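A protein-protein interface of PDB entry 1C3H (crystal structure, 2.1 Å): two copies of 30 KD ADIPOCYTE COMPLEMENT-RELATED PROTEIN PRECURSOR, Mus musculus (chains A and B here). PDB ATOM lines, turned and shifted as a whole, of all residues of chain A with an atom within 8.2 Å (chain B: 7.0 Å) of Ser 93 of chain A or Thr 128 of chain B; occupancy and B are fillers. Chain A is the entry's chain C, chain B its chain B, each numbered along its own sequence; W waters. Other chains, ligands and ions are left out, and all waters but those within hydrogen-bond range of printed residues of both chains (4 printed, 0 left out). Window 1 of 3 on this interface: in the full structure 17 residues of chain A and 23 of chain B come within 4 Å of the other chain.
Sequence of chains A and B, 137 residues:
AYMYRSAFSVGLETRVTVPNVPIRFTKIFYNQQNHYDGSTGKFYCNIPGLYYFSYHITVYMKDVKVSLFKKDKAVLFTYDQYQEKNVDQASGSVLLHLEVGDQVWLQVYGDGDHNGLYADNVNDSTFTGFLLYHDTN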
ATOM      1  N   LEU A  50      -3.935  -5.956  -8.295  1.00  0.00           N
ATOM      2  CA  LEU A  50      -5.133  -6.388  -8.994  1.00  0.00           C
ATOM      3  C   LEU A  50      -6.339  -5.616  -8.483  1.00  0.00           C
ATOM      4  O   LEU A  50      -6.643  -5.622  -7.285  1.00  0.00           O
ATOM      5  CB  LEU A  50      -5.357  -7.880  -8.758  1.00  0.00           C
ATOM      6  CG  LEU A  50      -5.971  -8.780  -9.833  1.00  0.00           C
ATOM      7  CD1 LEU A  50      -6.854  -9.791  -9.129  1.00  0.00           C
ATOM      8  CD2 LEU A  50      -6.749  -7.999 -10.869  1.00  0.00           C
ATOM      9  N   TYR A  51      -7.030  -4.962  -9.401  1.00  0.00           N
ATOM     10  CA  TYR A  51      -8.202  -4.181  -9.054  1.00  0.00           C
ATOM     11  C   TYR A  51      -9.449  -4.792  -9.647  1.00  0.00           C
ATOM     12  O   TYR A  51      -9.392  -5.453 -10.677  1.00  0.00           O
ATOM     13  CB  TYR A  51      -8.074  -2.751  -9.578  1.00  0.00           C
ATOM     14  CG  TYR A  51      -7.070  -1.915  -8.841  1.00  0.00           C
ATOM     15  CD1 TYR A  51      -5.704  -2.092  -9.039  1.00  0.00           C
ATOM     16  CD2 TYR A  51      -7.485  -0.964  -7.915  1.00  0.00           C
ATOM     17  CE1 TYR A  51      -4.775  -1.337  -8.323  1.00  0.00           C
ATOM     18  CE2 TYR A  51      -6.579  -0.217  -7.204  1.00  0.00           C
ATOM     19  CZ  TYR A  51      -5.217  -0.406  -7.410  1.00  0.00           C
ATOM     20  OH  TYR A  51      -4.310   0.337  -6.685  1.00  0.00           O
ATOM     21  N   TYR A  52     -10.575  -4.560  -8.988  1.00  0.00           N
ATOM     22  CA  TYR A  52     -11.861  -5.046  -9.477  1.00  0.00           C
ATOM     23  C   TYR A  52     -12.600  -3.771  -9.848  1.00  0.00           C
ATOM     24  O   TYR A  52     -12.556  -2.805  -9.102  1.00  0.00           O
ATOM     25  CB  TYR A  52     -12.648  -5.784  -8.375  1.00  0.00           C
ATOM     26  CG  TYR A  52     -14.000  -6.308  -8.841  1.00  0.00           C
ATOM     27  CD1 TYR A  52     -14.083  -7.338  -9.768  1.00  0.00           C
ATOM     28  CD2 TYR A  52     -15.187  -5.753  -8.376  1.00  0.00           C
ATOM     29  CE1 TYR A  52     -15.322  -7.804 -10.230  1.00  0.00           C
ATOM     30  CE2 TYR A  52     -16.438  -6.212  -8.829  1.00  0.00           C
ATOM     31  CZ  TYR A  52     -16.493  -7.236  -9.759  1.00  0.00           C
ATOM     32  OH  TYR A  52     -17.711  -7.687 -10.244  1.00  0.00           O
ATOM     33  N   PHE A  53     -13.244  -3.759 -11.009  1.00  0.00           N
ATOM     34  CA  PHE A  53     -14.011  -2.598 -11.444  1.00  0.00           C
ATOM     35  C   PHE A  53     -15.408  -3.041 -11.796  1.00  0.00           C
ATOM     36  O   PHE A  53     -15.612  -4.129 -12.324  1.00  0.00           O
ATOM     37  CB  PHE A  53     -13.374  -1.912 -12.664  1.00  0.00           C
ATOM     38  CG  PHE A  53     -12.130  -1.154 -12.338  1.00  0.00           C
ATOM     39  CD1 PHE A  53     -10.880  -1.756 -12.456  1.00  0.00           C
ATOM     40  CD2 PHE A  53     -12.211   0.143 -11.850  1.00  0.00           C
ATOM     41  CE1 PHE A  53      -9.722  -1.073 -12.088  1.00  0.00           C
ATOM     42  CE2 PHE A  53     -11.055   0.840 -11.476  1.00  0.00           C
ATOM     43  CZ  PHE A  53      -9.806   0.223 -11.595  1.00  0.00           C
ATOM     44  N   SER A  54     -16.370  -2.183 -11.497  1.00  0.00           N
ATOM     45  CA  SER A  54     -17.766  -2.486 -11.767  1.00  0.00           C
ATOM     46  C   SER A  54     -18.489  -1.192 -12.069  1.00  0.00           C
ATOM     47  O   SER A  54     -18.232  -0.173 -11.429  1.00  0.00           O
ATOM     48  CB  SER A  54     -18.413  -3.147 -10.539  1.00  0.00           C
ATOM     49  OG  SER A  54     -19.790  -3.411 -10.775  1.00  0.00           O
ATOM     50  N   TYR A  55     -19.397  -1.231 -13.033  1.00  0.00           N
ATOM     51  CA  TYR A  55     -20.143  -0.035 -13.376  1.00  0.00           C
ATOM     52  C   TYR A  55     -21.538  -0.398 -13.858  1.00  0.00           C
ATOM     53  O   TYR A  55     -21.766  -1.487 -14.376  1.00  0.00           O
ATOM     54  CB  TYR A  55     -19.411   0.764 -14.461  1.00  0.00           C
ATOM     55  CG  TYR A  55     -19.284   0.033 -15.775  1.00  0.00           C
ATOM     56  CD1 TYR A  55     -20.325   0.027 -16.697  1.00  0.00           C
ATOM     57  CD2 TYR A  55     -18.120  -0.662 -16.093  1.00  0.00           C
ATOM     58  CE1 TYR A  55     -20.210  -0.649 -17.902  1.00  0.00           C
ATOM     59  CE2 TYR A  55     -17.996  -1.341 -17.292  1.00  0.00           C
ATOM     60  CZ  TYR A  55     -19.043  -1.330 -18.191  1.00  0.00           C
ATOM     61  OH  TYR A  55     -18.923  -2.021 -19.378  1.00  0.00           O
ATOM     62  N   HIS A  56     -22.458   0.535 -13.665  1.00  0.00           N
ATOM     63  CA  HIS A  56     -23.853   0.381 -14.071  1.00  0.00           C
ATOM     64  C   HIS A  56     -24.243   1.788 -14.483  1.00  0.00           C
ATOM     65  O   HIS A  56     -24.393   2.662 -13.639  1.00  0.00           O
ATOM     66  CB  HIS A  56     -24.711  -0.064 -12.886  1.00  0.00           C
ATOM     67  CG  HIS A  56     -24.276  -1.361 -12.279  1.00  0.00           C
ATOM     68  ND1 HIS A  56     -24.635  -2.586 -12.800  1.00  0.00           N
ATOM     69  CD2 HIS A  56     -23.504  -1.623 -11.197  1.00  0.00           C
ATOM     70  CE1 HIS A  56     -24.108  -3.548 -12.063  1.00  0.00           C
ATOM     71  NE2 HIS A  56     -23.417  -2.990 -11.082  1.00  0.00           N
ATOM     72  N   LEU A  68     -14.628   0.871 -21.267  1.00  0.00           N
ATOM     73  CA  LEU A  68     -13.937   1.030 -20.002  1.00  0.00           C
ATOM     74  C   LEU A  68     -12.503   1.186 -20.498  1.00  0.00           C
ATOM     75  O   LEU A  68     -12.000   0.336 -21.230  1.00  0.00           O
ATOM     76  CB  LEU A  68     -14.092  -0.228 -19.139  1.00  0.00           C
ATOM     77  CG  LEU A  68     -13.555  -0.239 -17.702  1.00  0.00           C
ATOM     78  CD1 LEU A  68     -12.178  -0.847 -17.679  1.00  0.00           C
ATOM     79  CD2 LEU A  68     -13.557   1.159 -17.110  1.00  0.00           C
ATOM     80  N   LEU A  76     -12.283  -2.841 -22.130  1.00  0.00           N
ATOM     81  CA  LEU A  76     -13.593  -3.479 -22.089  1.00  0.00           C
ATOM     82  C   LEU A  76     -14.524  -2.696 -23.021  1.00  0.00           C
ATOM     83  O   LEU A  76     -14.567  -1.470 -22.978  1.00  0.00           O
ATOM     84  CB  LEU A  76     -14.121  -3.466 -20.650  1.00  0.00           C
ATOM     85  CG  LEU A  76     -15.293  -4.369 -20.252  1.00  0.00           C
ATOM     86  CD1 LEU A  76     -16.547  -3.963 -21.004  1.00  0.00           C
ATOM     87  CD2 LEU A  76     -14.931  -5.817 -20.540  1.00  0.00           C
ATOM     88  N   THR A  78     -18.526  -2.485 -24.382  1.00  0.00           N
ATOM     89  CA  THR A  78     -19.920  -2.904 -24.282  1.00  0.00           C
ATOM     90  C   THR A  78     -20.791  -2.284 -25.369  1.00  0.00           C
ATOM     91  O   THR A  78     -20.769  -1.077 -25.594  1.00  0.00           O
ATOM     92  CB  THR A  78     -20.522  -2.527 -22.903  1.00  0.00           C
ATOM     93  OG1 THR A  78     -19.830  -3.232 -21.864  1.00  0.00           O
ATOM     94  CG2 THR A  78     -21.999  -2.885 -22.847  1.00  0.00           C
ATOM     95  N   SER A  91     -23.752  -2.288 -18.133  1.00  0.00           N
ATOM     96  CA  SER A  91     -23.074  -2.636 -16.897  1.00  0.00           C
ATOM     97  C   SER A  91     -21.946  -3.597 -17.229  1.00  0.00           C
ATOM     98  O   SER A  91     -21.961  -4.246 -18.271  1.00  0.00           O
ATOM     99  CB  SER A  91     -24.044  -3.289 -15.902  1.00  0.00           C
ATOM    100  OG  SER A  91     -24.460  -4.564 -16.355  1.00  0.00           O
ATOM    101  N   GLY A  92     -20.960  -3.670 -16.349  1.00  0.00           N
ATOM    102  CA  GLY A  92     -19.846  -4.563 -16.582  1.00  0.00           C
ATOM    103  C   GLY A  92     -18.950  -4.639 -15.369  1.00  0.00           C
ATOM    104  O   GLY A  92     -19.007  -3.798 -14.491  1.00  0.00           O
ATOM    105  N   SER A  93     -18.126  -5.670 -15.308  1.00  0.00           N
ATOM    106  CA  SER A  93     -17.213  -5.814 -14.195  1.00  0.00           C
ATOM    107  C   SER A  93     -16.013  -6.530 -14.760  1.00  0.00           C
ATOM    108  O   SER A  93     -16.136  -7.308 -15.706  1.00  0.00           O
ATOM    109  CB  SER A  93     -17.854  -6.630 -13.065  1.00  0.00           C
ATOM    110  OG  SER A  93     -18.139  -7.948 -13.477  1.00  0.00           O
ATOM    111  N   VAL A  94     -14.845  -6.261 -14.194  1.00  0.00           N
ATOM    112  CA  VAL A  94     -13.641  -6.893 -14.687  1.00  0.00           C
ATOM    113  C   VAL A  94     -12.520  -6.688 -13.688  1.00  0.00           C
ATOM    114  O   VAL A  94     -12.587  -5.796 -12.847  1.00  0.00           O
ATOM    115  CB  VAL A  94     -13.214  -6.265 -16.044  1.00  0.00           C
ATOM    116  CG1 VAL A  94     -12.765  -4.816 -15.823  1.00  0.00           C
ATOM    117  CG2 VAL A  94     -12.109  -7.100 -16.697  1.00  0.00           C
ATOM    118  N   LEU A  95     -11.502  -7.532 -13.787  1.00  0.00           N
ATOM    119  CA  LEU A  95     -10.326  -7.440 -12.936  1.00  0.00           C
ATOM    120  C   LEU A  95      -9.213  -6.950 -13.846  1.00  0.00           C
ATOM    121  O   LEU A  95      -9.035  -7.477 -14.940  1.00  0.00           O
ATOM    122  CB  LEU A  95      -9.934  -8.812 -12.374  1.00  0.00           C
ATOM    123  CG  LEU A  95     -10.731  -9.419 -11.216  1.00  0.00           C
ATOM    124  CD1 LEU A  95     -10.292 -10.863 -11.035  1.00  0.00           C
ATOM    125  CD2 LEU A  95     -10.509  -8.628  -9.925  1.00  0.00           C
ATOM    126  N   LEU A  96      -8.483  -5.935 -13.399  1.00  0.00           N
ATOM    127  CA  LEU A  96      -7.381  -5.383 -14.174  1.00  0.00           C
ATOM    128  C   LEU A  96      -6.176  -5.222 -13.284  1.00  0.00           C
ATOM    129  O   LEU A  96      -6.290  -4.690 -12.172  1.00  0.00           O
ATOM    130  CB  LEU A  96      -7.738  -4.001 -14.719  1.00  0.00           C
ATOM    131  CG  LEU A  96      -8.911  -3.836 -15.681  1.00  0.00           C
ATOM    132  CD1 LEU A  96      -9.065  -2.368 -16.012  1.00  0.00           C
ATOM    133  CD2 LEU A  96      -8.671  -4.647 -16.928  1.00  0.00           C
ATOM    134  N   THR A 128     -17.461   1.845  -9.834  1.00  0.00           N
ATOM    135  CA  THR A 128     -16.763   1.423  -8.624  1.00  0.00           C
ATOM    136  C   THR A 128     -15.483   0.645  -8.912  1.00  0.00           C
ATOM    137  O   THR A 128     -15.360  -0.001  -9.936  1.00  0.00           O
ATOM    138  CB  THR A 128     -17.703   0.526  -7.753  1.00  0.00           C
ATOM    139  OG1 THR A 128     -18.918   1.235  -7.484  1.00  0.00           O
ATOM    140  CG2 THR A 128     -17.029   0.155  -6.419  1.00  0.00           C
ATOM    141  N   LEU A 132      -7.748  -5.311  -4.929  1.00  0.00           N
ATOM    142  CA  LEU A 132      -8.007  -6.642  -4.415  1.00  0.00           C
ATOM    143  C   LEU A 132      -6.698  -7.147  -3.804  1.00  0.00           C
ATOM    144  O   LEU A 132      -6.621  -7.422  -2.601  1.00  0.00           O
ATOM    145  CB  LEU A 132      -8.417  -7.569  -5.561  1.00  0.00           C
ATOM    146  CG  LEU A 132      -9.474  -8.652  -5.345  1.00  0.00           C
ATOM    147  CD1 LEU A 132      -9.304  -9.701  -6.439  1.00  0.00           C
ATOM    148  CD2 LEU A 132      -9.344  -9.299  -3.973  1.00  0.00           C
ATOM    149  N   ALA B   7      -7.627 -15.505  -8.528  1.00  0.00           N
ATOM    150  CA  ALA B   7      -8.579 -14.650  -9.206  1.00  0.00           C
ATOM    151  C   ALA B   7      -8.446 -14.813 -10.705  1.00  0.00           C
ATOM    152  O   ALA B   7      -7.392 -15.208 -11.212  1.00  0.00           O
ATOM    153  CB  ALA B   7      -8.329 -13.202  -8.824  1.00  0.00           C
ATOM    154  N   PHE B   8      -9.523 -14.518 -11.414  1.00  0.00           N
ATOM    155  CA  PHE B   8      -9.501 -14.618 -12.857  1.00  0.00           C
ATOM    156  C   PHE B   8     -10.572 -13.711 -13.411  1.00  0.00           C
ATOM    157  O   PHE B   8     -11.580 -13.444 -12.755  1.00  0.00           O
ATOM    158  CB  PHE B   8      -9.754 -16.062 -13.305  1.00  0.00           C
ATOM    159  CG  PHE B   8     -11.183 -16.498 -13.154  1.00  0.00           C
ATOM    160  CD1 PHE B   8     -12.096 -16.297 -14.181  1.00  0.00           C
ATOM    161  CD2 PHE B   8     -11.634 -17.046 -11.954  1.00  0.00           C
ATOM    162  CE1 PHE B   8     -13.445 -16.629 -14.015  1.00  0.00           C
ATOM    163  CE2 PHE B   8     -12.978 -17.379 -11.783  1.00  0.00           C
ATOM    164  CZ  PHE B   8     -13.882 -17.165 -12.822  1.00  0.00           C
ATOM    165  N   SER B   9     -10.332 -13.215 -14.615  1.00  0.00           N
ATOM    166  CA  SER B   9     -11.282 -12.364 -15.290  1.00  0.00           C
ATOM    167  C   SER B   9     -11.034 -12.677 -16.762  1.00  0.00           C
ATOM    168  O   SER B   9      -9.936 -12.450 -17.271  1.00  0.00           O
ATOM    169  CB  SER B   9     -10.998 -10.901 -14.966  1.00  0.00           C
ATOM    170  OG  SER B   9     -12.058 -10.079 -15.395  1.00  0.00           O
ATOM    171  N   VAL B  10     -12.052 -13.223 -17.419  1.00  0.00           N
ATOM    172  CA  VAL B  10     -11.963 -13.626 -18.815  1.00  0.00           C
ATOM    173  C   VAL B  10     -13.197 -13.222 -19.621  1.00  0.00           C
ATOM    174  O   VAL B  10     -14.281 -13.024 -19.061  1.00  0.00           O
ATOM    175  CB  VAL B  10     -11.787 -15.154 -18.915  1.00  0.00           C
ATOM    176  CG1 VAL B  10     -10.512 -15.567 -18.209  1.00  0.00           C
ATOM    177  CG2 VAL B  10     -12.985 -15.860 -18.276  1.00  0.00           C
ATOM    178  N   PHE B  29      -8.289 -11.247 -19.279  1.00  0.00           N
ATOM    179  CA  PHE B  29      -8.037  -9.948 -18.662  1.00  0.00           C
ATOM    180  C   PHE B  29      -7.105 -10.207 -17.487  1.00  0.00           C
ATOM    181  O   PHE B  29      -6.257  -9.378 -17.141  1.00  0.00           O
ATOM    182  CB  PHE B  29      -9.338  -9.304 -18.167  1.00  0.00           C
ATOM    183  CG  PHE B  29     -10.340  -9.058 -19.255  1.00  0.00           C
ATOM    184  CD1 PHE B  29     -11.266 -10.035 -19.600  1.00  0.00           C
ATOM    185  CD2 PHE B  29     -10.346  -7.854 -19.949  1.00  0.00           C
ATOM    186  CE1 PHE B  29     -12.184  -9.816 -20.621  1.00  0.00           C
ATOM    187  CE2 PHE B  29     -11.264  -7.625 -20.975  1.00  0.00           C
ATOM    188  CZ  PHE B  29     -12.183  -8.610 -21.309  1.00  0.00           C
ATOM    189  N   TYR B  52     -16.030 -14.641  -4.742  1.00  0.00           N
ATOM    190  CA  TYR B  52     -17.047 -13.782  -5.320  1.00  0.00           C
ATOM    191  C   TYR B  52     -16.961 -14.053  -6.813  1.00  0.00           C
ATOM    192  O   TYR B  52     -15.856 -14.166  -7.364  1.00  0.00           O
ATOM    193  CB  TYR B  52     -16.752 -12.304  -5.050  1.00  0.00           C
ATOM    194  CG  TYR B  52     -17.784 -11.351  -5.627  1.00  0.00           C
ATOM    195  CD1 TYR B  52     -19.091 -11.335  -5.144  1.00  0.00           C
ATOM    196  CD2 TYR B  52     -17.448 -10.451  -6.637  1.00  0.00           C
ATOM    197  CE1 TYR B  52     -20.037 -10.446  -5.648  1.00  0.00           C
ATOM    198  CE2 TYR B  52     -18.386  -9.552  -7.152  1.00  0.00           C
ATOM    199  CZ  TYR B  52     -19.682  -9.556  -6.651  1.00  0.00           C
ATOM    200  OH  TYR B  52     -20.632  -8.686  -7.156  1.00  0.00           O
ATOM    201  N   PHE B  53     -18.117 -14.198  -7.452  1.00  0.00           N
ATOM    202  CA  PHE B  53     -18.186 -14.411  -8.891  1.00  0.00           C
ATOM    203  C   PHE B  53     -19.129 -13.385  -9.480  1.00  0.00           C
ATOM    204  O   PHE B  53     -20.095 -12.954  -8.833  1.00  0.00           O
ATOM    205  CB  PHE B  53     -18.689 -15.815  -9.252  1.00  0.00           C
ATOM    206  CG  PHE B  53     -17.715 -16.903  -8.932  1.00  0.00           C
ATOM    207  CD1 PHE B  53     -17.747 -17.542  -7.694  1.00  0.00           C
ATOM    208  CD2 PHE B  53     -16.733 -17.264  -9.850  1.00  0.00           C
ATOM    209  CE1 PHE B  53     -16.810 -18.529  -7.373  1.00  0.00           C
ATOM    210  CE2 PHE B  53     -15.791 -18.250  -9.541  1.00  0.00           C
ATOM    211  CZ  PHE B  53     -15.832 -18.882  -8.295  1.00  0.00           C
ATOM    212  N   SER B  54     -18.838 -12.999 -10.716  1.00  0.00           N
ATOM    213  CA  SER B  54     -19.627 -12.008 -11.423  1.00  0.00           C
ATOM    214  C   SER B  54     -19.491 -12.251 -12.920  1.00  0.00           C
ATOM    215  O   SER B  54     -18.398 -12.525 -13.426  1.00  0.00           O
ATOM    216  CB  SER B  54     -19.133 -10.599 -11.080  1.00  0.00           C
ATOM    217  OG  SER B  54     -19.703  -9.623 -11.943  1.00  0.00           O
ATOM    218  N   TYR B  55     -20.605 -12.165 -13.625  1.00  0.00           N
ATOM    219  CA  TYR B  55     -20.572 -12.366 -15.062  1.00  0.00           C
ATOM    220  C   TYR B  55     -21.530 -11.411 -15.733  1.00  0.00           C
ATOM    221  O   TYR B  55     -22.500 -10.947 -15.120  1.00  0.00           O
ATOM    222  CB  TYR B  55     -20.920 -13.814 -15.418  1.00  0.00           C
ATOM    223  CG  TYR B  55     -22.308 -14.238 -15.003  1.00  0.00           C
ATOM    224  CD1 TYR B  55     -23.424 -13.911 -15.772  1.00  0.00           C
ATOM    225  CD2 TYR B  55     -22.508 -14.944 -13.824  1.00  0.00           C
ATOM    226  CE1 TYR B  55     -24.705 -14.275 -15.367  1.00  0.00           C
ATOM    227  CE2 TYR B  55     -23.773 -15.310 -13.415  1.00  0.00           C
ATOM    228  CZ  TYR B  55     -24.867 -14.971 -14.185  1.00  0.00           C
ATOM    229  OH  TYR B  55     -26.122 -15.310 -13.742  1.00  0.00           O
ATOM    230  N   HIS B  56     -21.226 -11.109 -16.992  1.00  0.00           N
ATOM    231  CA  HIS B  56     -22.016 -10.215 -17.820  1.00  0.00           C
ATOM    232  C   HIS B  56     -21.846 -10.806 -19.204  1.00  0.00           C
ATOM    233  O   HIS B  56     -20.809 -10.623 -19.836  1.00  0.00           O
ATOM    234  CB  HIS B  56     -21.433  -8.803 -17.805  1.00  0.00           C
ATOM    235  CG  HIS B  56     -21.393  -8.175 -16.449  1.00  0.00           C
ATOM    236  ND1 HIS B  56     -22.479  -7.536 -15.892  1.00  0.00           N
ATOM    237  CD2 HIS B  56     -20.392  -8.076 -15.543  1.00  0.00           C
ATOM    238  CE1 HIS B  56     -22.147  -7.066 -14.702  1.00  0.00           C
ATOM    239  NE2 HIS B  56     -20.886  -7.380 -14.467  1.00  0.00           N
ATOM    240  N   GLY B  92     -24.925 -11.422 -13.393  1.00  0.00           N
ATOM    241  CA  GLY B  92     -25.147 -11.981 -12.074  1.00  0.00           C
ATOM    242  C   GLY B  92     -23.903 -11.933 -11.211  1.00  0.00           C
ATOM    243  O   GLY B  92     -22.783 -11.823 -11.710  1.00  0.00           O
ATOM    244  N   LEU B 106     -19.869 -21.219 -16.420  1.00  0.00           N
ATOM    245  CA  LEU B 106     -21.144 -20.701 -16.882  1.00  0.00           C
ATOM    246  C   LEU B 106     -21.650 -21.596 -17.996  1.00  0.00           C
ATOM    247  O   LEU B 106     -20.870 -22.213 -18.718  1.00  0.00           O
ATOM    248  CB  LEU B 106     -20.991 -19.266 -17.376  1.00  0.00           C
ATOM    249  CG  LEU B 106     -20.728 -18.252 -16.265  1.00  0.00           C
ATOM    250  CD1 LEU B 106     -20.408 -16.895 -16.874  1.00  0.00           C
ATOM    251  CD2 LEU B 106     -21.957 -18.165 -15.351  1.00  0.00           C
ATOM    252  N   THR B 126     -18.162 -11.098 -20.044  1.00  0.00           N
ATOM    253  CA  THR B 126     -17.145 -11.414 -19.048  1.00  0.00           C
ATOM    254  C   THR B 126     -17.559 -12.372 -17.936  1.00  0.00           C
ATOM    255  O   THR B 126     -18.731 -12.491 -17.588  1.00  0.00           O
ATOM    256  CB  THR B 126     -16.617 -10.130 -18.365  1.00  0.00           C
ATOM    257  OG1 THR B 126     -17.687  -9.498 -17.656  1.00  0.00           O
ATOM    258  CG2 THR B 126     -16.058  -9.156 -19.396  1.00  0.00           C
ATOM    259  N   PHE B 127     -16.555 -13.044 -17.386  1.00  0.00           N
ATOM    260  CA  PHE B 127     -16.729 -13.983 -16.292  1.00  0.00           C
ATOM    261  C   PHE B 127     -15.558 -13.688 -15.378  1.00  0.00           C
ATOM    262  O   PHE B 127     -14.399 -13.799 -15.784  1.00  0.00           O
ATOM    263  CB  PHE B 127     -16.672 -15.416 -16.814  1.00  0.00           C
ATOM    264  CG  PHE B 127     -16.876 -16.460 -15.754  1.00  0.00           C
ATOM    265  CD1 PHE B 127     -17.699 -16.212 -14.658  1.00  0.00           C
ATOM    266  CD2 PHE B 127     -16.278 -17.714 -15.879  1.00  0.00           C
ATOM    267  CE1 PHE B 127     -17.932 -17.202 -13.694  1.00  0.00           C
ATOM    268  CE2 PHE B 127     -16.502 -18.714 -14.923  1.00  0.00           C
ATOM    269  CZ  PHE B 127     -17.331 -18.456 -13.830  1.00  0.00           C
ATOM    270  N   THR B 128     -15.870 -13.299 -14.147  1.00  0.00           N
ATOM    271  CA  THR B 128     -14.853 -12.921 -13.182  1.00  0.00           C
ATOM    272  C   THR B 128     -15.063 -13.617 -11.845  1.00  0.00           C
ATOM    273  O   THR B 128     -16.182 -13.952 -11.475  1.00  0.00           O
ATOM    274  CB  THR B 128     -14.880 -11.383 -12.964  1.00  0.00           C
ATOM    275  OG1 THR B 128     -14.697 -10.723 -14.225  1.00  0.00           O
ATOM    276  CG2 THR B 128     -13.780 -10.949 -12.000  1.00  0.00           C
ATOM    277  N   GLY B 129     -13.975 -13.840 -11.125  1.00  0.00           N
ATOM    278  CA  GLY B 129     -14.073 -14.478  -9.831  1.00  0.00           C
ATOM    279  C   GLY B 129     -12.795 -14.266  -9.042  1.00  0.00           C
ATOM    280  O   GLY B 129     -11.724 -14.173  -9.625  1.00  0.00           O
ATOM    281  N   PHE B 130     -12.909 -14.153  -7.726  1.00  0.00           N
ATOM    282  CA  PHE B 130     -11.731 -14.002  -6.888  1.00  0.00           C
ATOM    283  C   PHE B 130     -11.989 -14.488  -5.472  1.00  0.00           C
ATOM    284  O   PHE B 130     -13.119 -14.472  -4.981  1.00  0.00           O
ATOM    285  CB  PHE B 130     -11.215 -12.555  -6.870  1.00  0.00           C
ATOM    286  CG  PHE B 130     -12.245 -11.526  -6.498  1.00  0.00           C
ATOM    287  CD1 PHE B 130     -12.486 -11.206  -5.172  1.00  0.00           C
ATOM    288  CD2 PHE B 130     -12.969 -10.861  -7.488  1.00  0.00           C
ATOM    289  CE1 PHE B 130     -13.429 -10.238  -4.823  1.00  0.00           C
ATOM    290  CE2 PHE B 130     -13.918  -9.889  -7.153  1.00  0.00           C
ATOM    291  CZ  PHE B 130     -14.146  -9.579  -5.821  1.00  0.00           C
HETATM  292  O   HOH W   1     -20.097  -6.786  -9.165  1.00  0.00           O
HETATM  293  O   HOH W   2     -17.173 -10.071 -14.909  1.00  0.00           O
HETATM  294  O   HOH W   3     -21.110  -4.808 -12.447  1.00  0.00           O
HETATM  295  O   HOH W   4     -18.227  -6.970 -17.918  1.00  0.00           O
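OG of Ser 54 of chain B sits at hydrogen-bond distance from OH of Tyr 52 of chain A, 3.3 Å away. A ring nitrogen (NE2) of His 56 of chain B lies within hydrogen-bond range of the side-chain hydroxyl (OG) of Ser 93 of chain A (3.0 Å). The side-chain hydroxyl (OG) of Ser 54 of chain B sits at hydrogen-bond distance from the side-chain hydroxyl (OG) of Ser 93 of chain A (2.8 Å). N of Leu 95 of chain A sits at hydrogen-bond distance from OG of Ser 9 of chain B, 3.1 Å away. OG1 of Thr 126 of chain B sits at hydrogen-bond distance from O of Ser 93 of chain A (3.3 Å).
OG of Ser 93 of chain A sits close to OH of Tyr 52 of chain A, at 3.3 Å. The backbone carbonyl oxygen (O) of Gly 92 of chain A sits at hydrogen-bond distance from the backbone NH (N) of Tyr 55 of chain A (3.0 Å). N of Phe 8 of chain B sits at hydrogen-bond distance from O of Gly 129 of chain B (2.9 Å). The backbone carbonyl oxygen of Phe 130 of chain B is in hydrogen-bond range of the backbone NH of Tyr 52 of chain B (2.9 Å).
Among the printed residues, pairs that only touch across the chains: Leu 50 of chain A with Ala 7 of chain B (3.7 Å), Tyr 52 of chain A with Tyr 52 of chain B (3.7 Å), Tyr 52 of chain A with Thr 128 of chain B (3.9 Å), Tyr 52 of chain A with Phe 130 of chain B (3.7 Å), Leu 76 of chain A with Phe 29 of chain B (3.99 Å), Leu 76 of chain A with Thr 126 of chain B (3.7 Å), Ser 91 of chain A with His 56 of chain B (3.6 Å), Gly 92 of chain A with His 56 of chain B (3.5 Å), Ser 93 of chain A with Thr 128 of chain B (3.99 Å), Val 94 of chain A with Ser 9 of chain B (3.3 Å), Val 94 of chain A with Phe 29 of chain B (3.7 Å), Val 94 of chain A with Thr 128 of chain B (3.9997 Å), Leu 95 of chain A with Ala 7 of chain B (3.8 Å), Leu 95 of chain A with Phe 8 of chain B (3.4 Å), Leu 95 of chain A with Phe 29 of chain B (3.7 Å), Leu 95 of chain A with Thr 128 of chain B (3.5 Å), Leu 95 of chain A with Gly 129 of chain B (3.9 Å) and Leu 132 of chain A with Phe 130 of chain B (3.5 Å).
Of the printed residues of chain A, Ser 9 of chain B touches Val 94 and Leu 95. Of the printed residues of chain A, Phe 29 of chain B touches Leu 76, Val 94 and Leu 95. Ser 54 of chain B touches two residues of chain A. Of the printed residues of chain A, Thr 128 of chain B touches Tyr 52 (3.9 Å), Ser 93 (3.99 Å), Val 94 (3.9997 Å) and Leu 95 (3.5 Å). Gly 129 of chain B touches just one residue of chain A: Leu 95. The nearest printed residue of chain B that does not touch Leu 95 of chain A is Phe 130 of chain B (4.1 Å).
Hydrophobic or aromatic side chains of chain B that line the printed part of chain A: Ala 7, Phe 29, Tyr 52, His 56 and Phe 130. Among the printed residues, 23 pairs touch across the chains. Among the printed residues, no Asp or Glu carboxylate lies within 4 Å of a Lys or Arg side-chain nitrogen of the other chain.
Tyr 52 of chain B touches its own counterpart, Tyr 52 of chain A. Tyr 52 of chain A touches Ser 54 of chain B, but with the chains exchanged Ser 54 of chain A does not touch Tyr 52 of chain B (6.5 Å). Gly 92 of chain A touches His 56 of chain B, but with the chains exchanged His 56 of chain A does not touch Gly 92 of chain B (8.0 Å). Positions printed for both chains: 52, 53, 54, 55, 56, 92 and 128.
Water W3 lies within hydrogen-bond range of OG of Ser 54 of chain A (2.5 Å), O of Gly 92 of chain A (3.1 Å), NE2 of His 56 of chain A (3.2 Å) and NE2 of His 56 of chain B (3.3 Å). Water W4 bridges the side-chain hydroxyl (OG1) of Thr 126 of chain B and the backbone NH (N) of Ser 93 of chain A. Water W1 lies within hydrogen-bond range of OH of Tyr 52 of chain A and OH of Tyr 52 of chain B.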
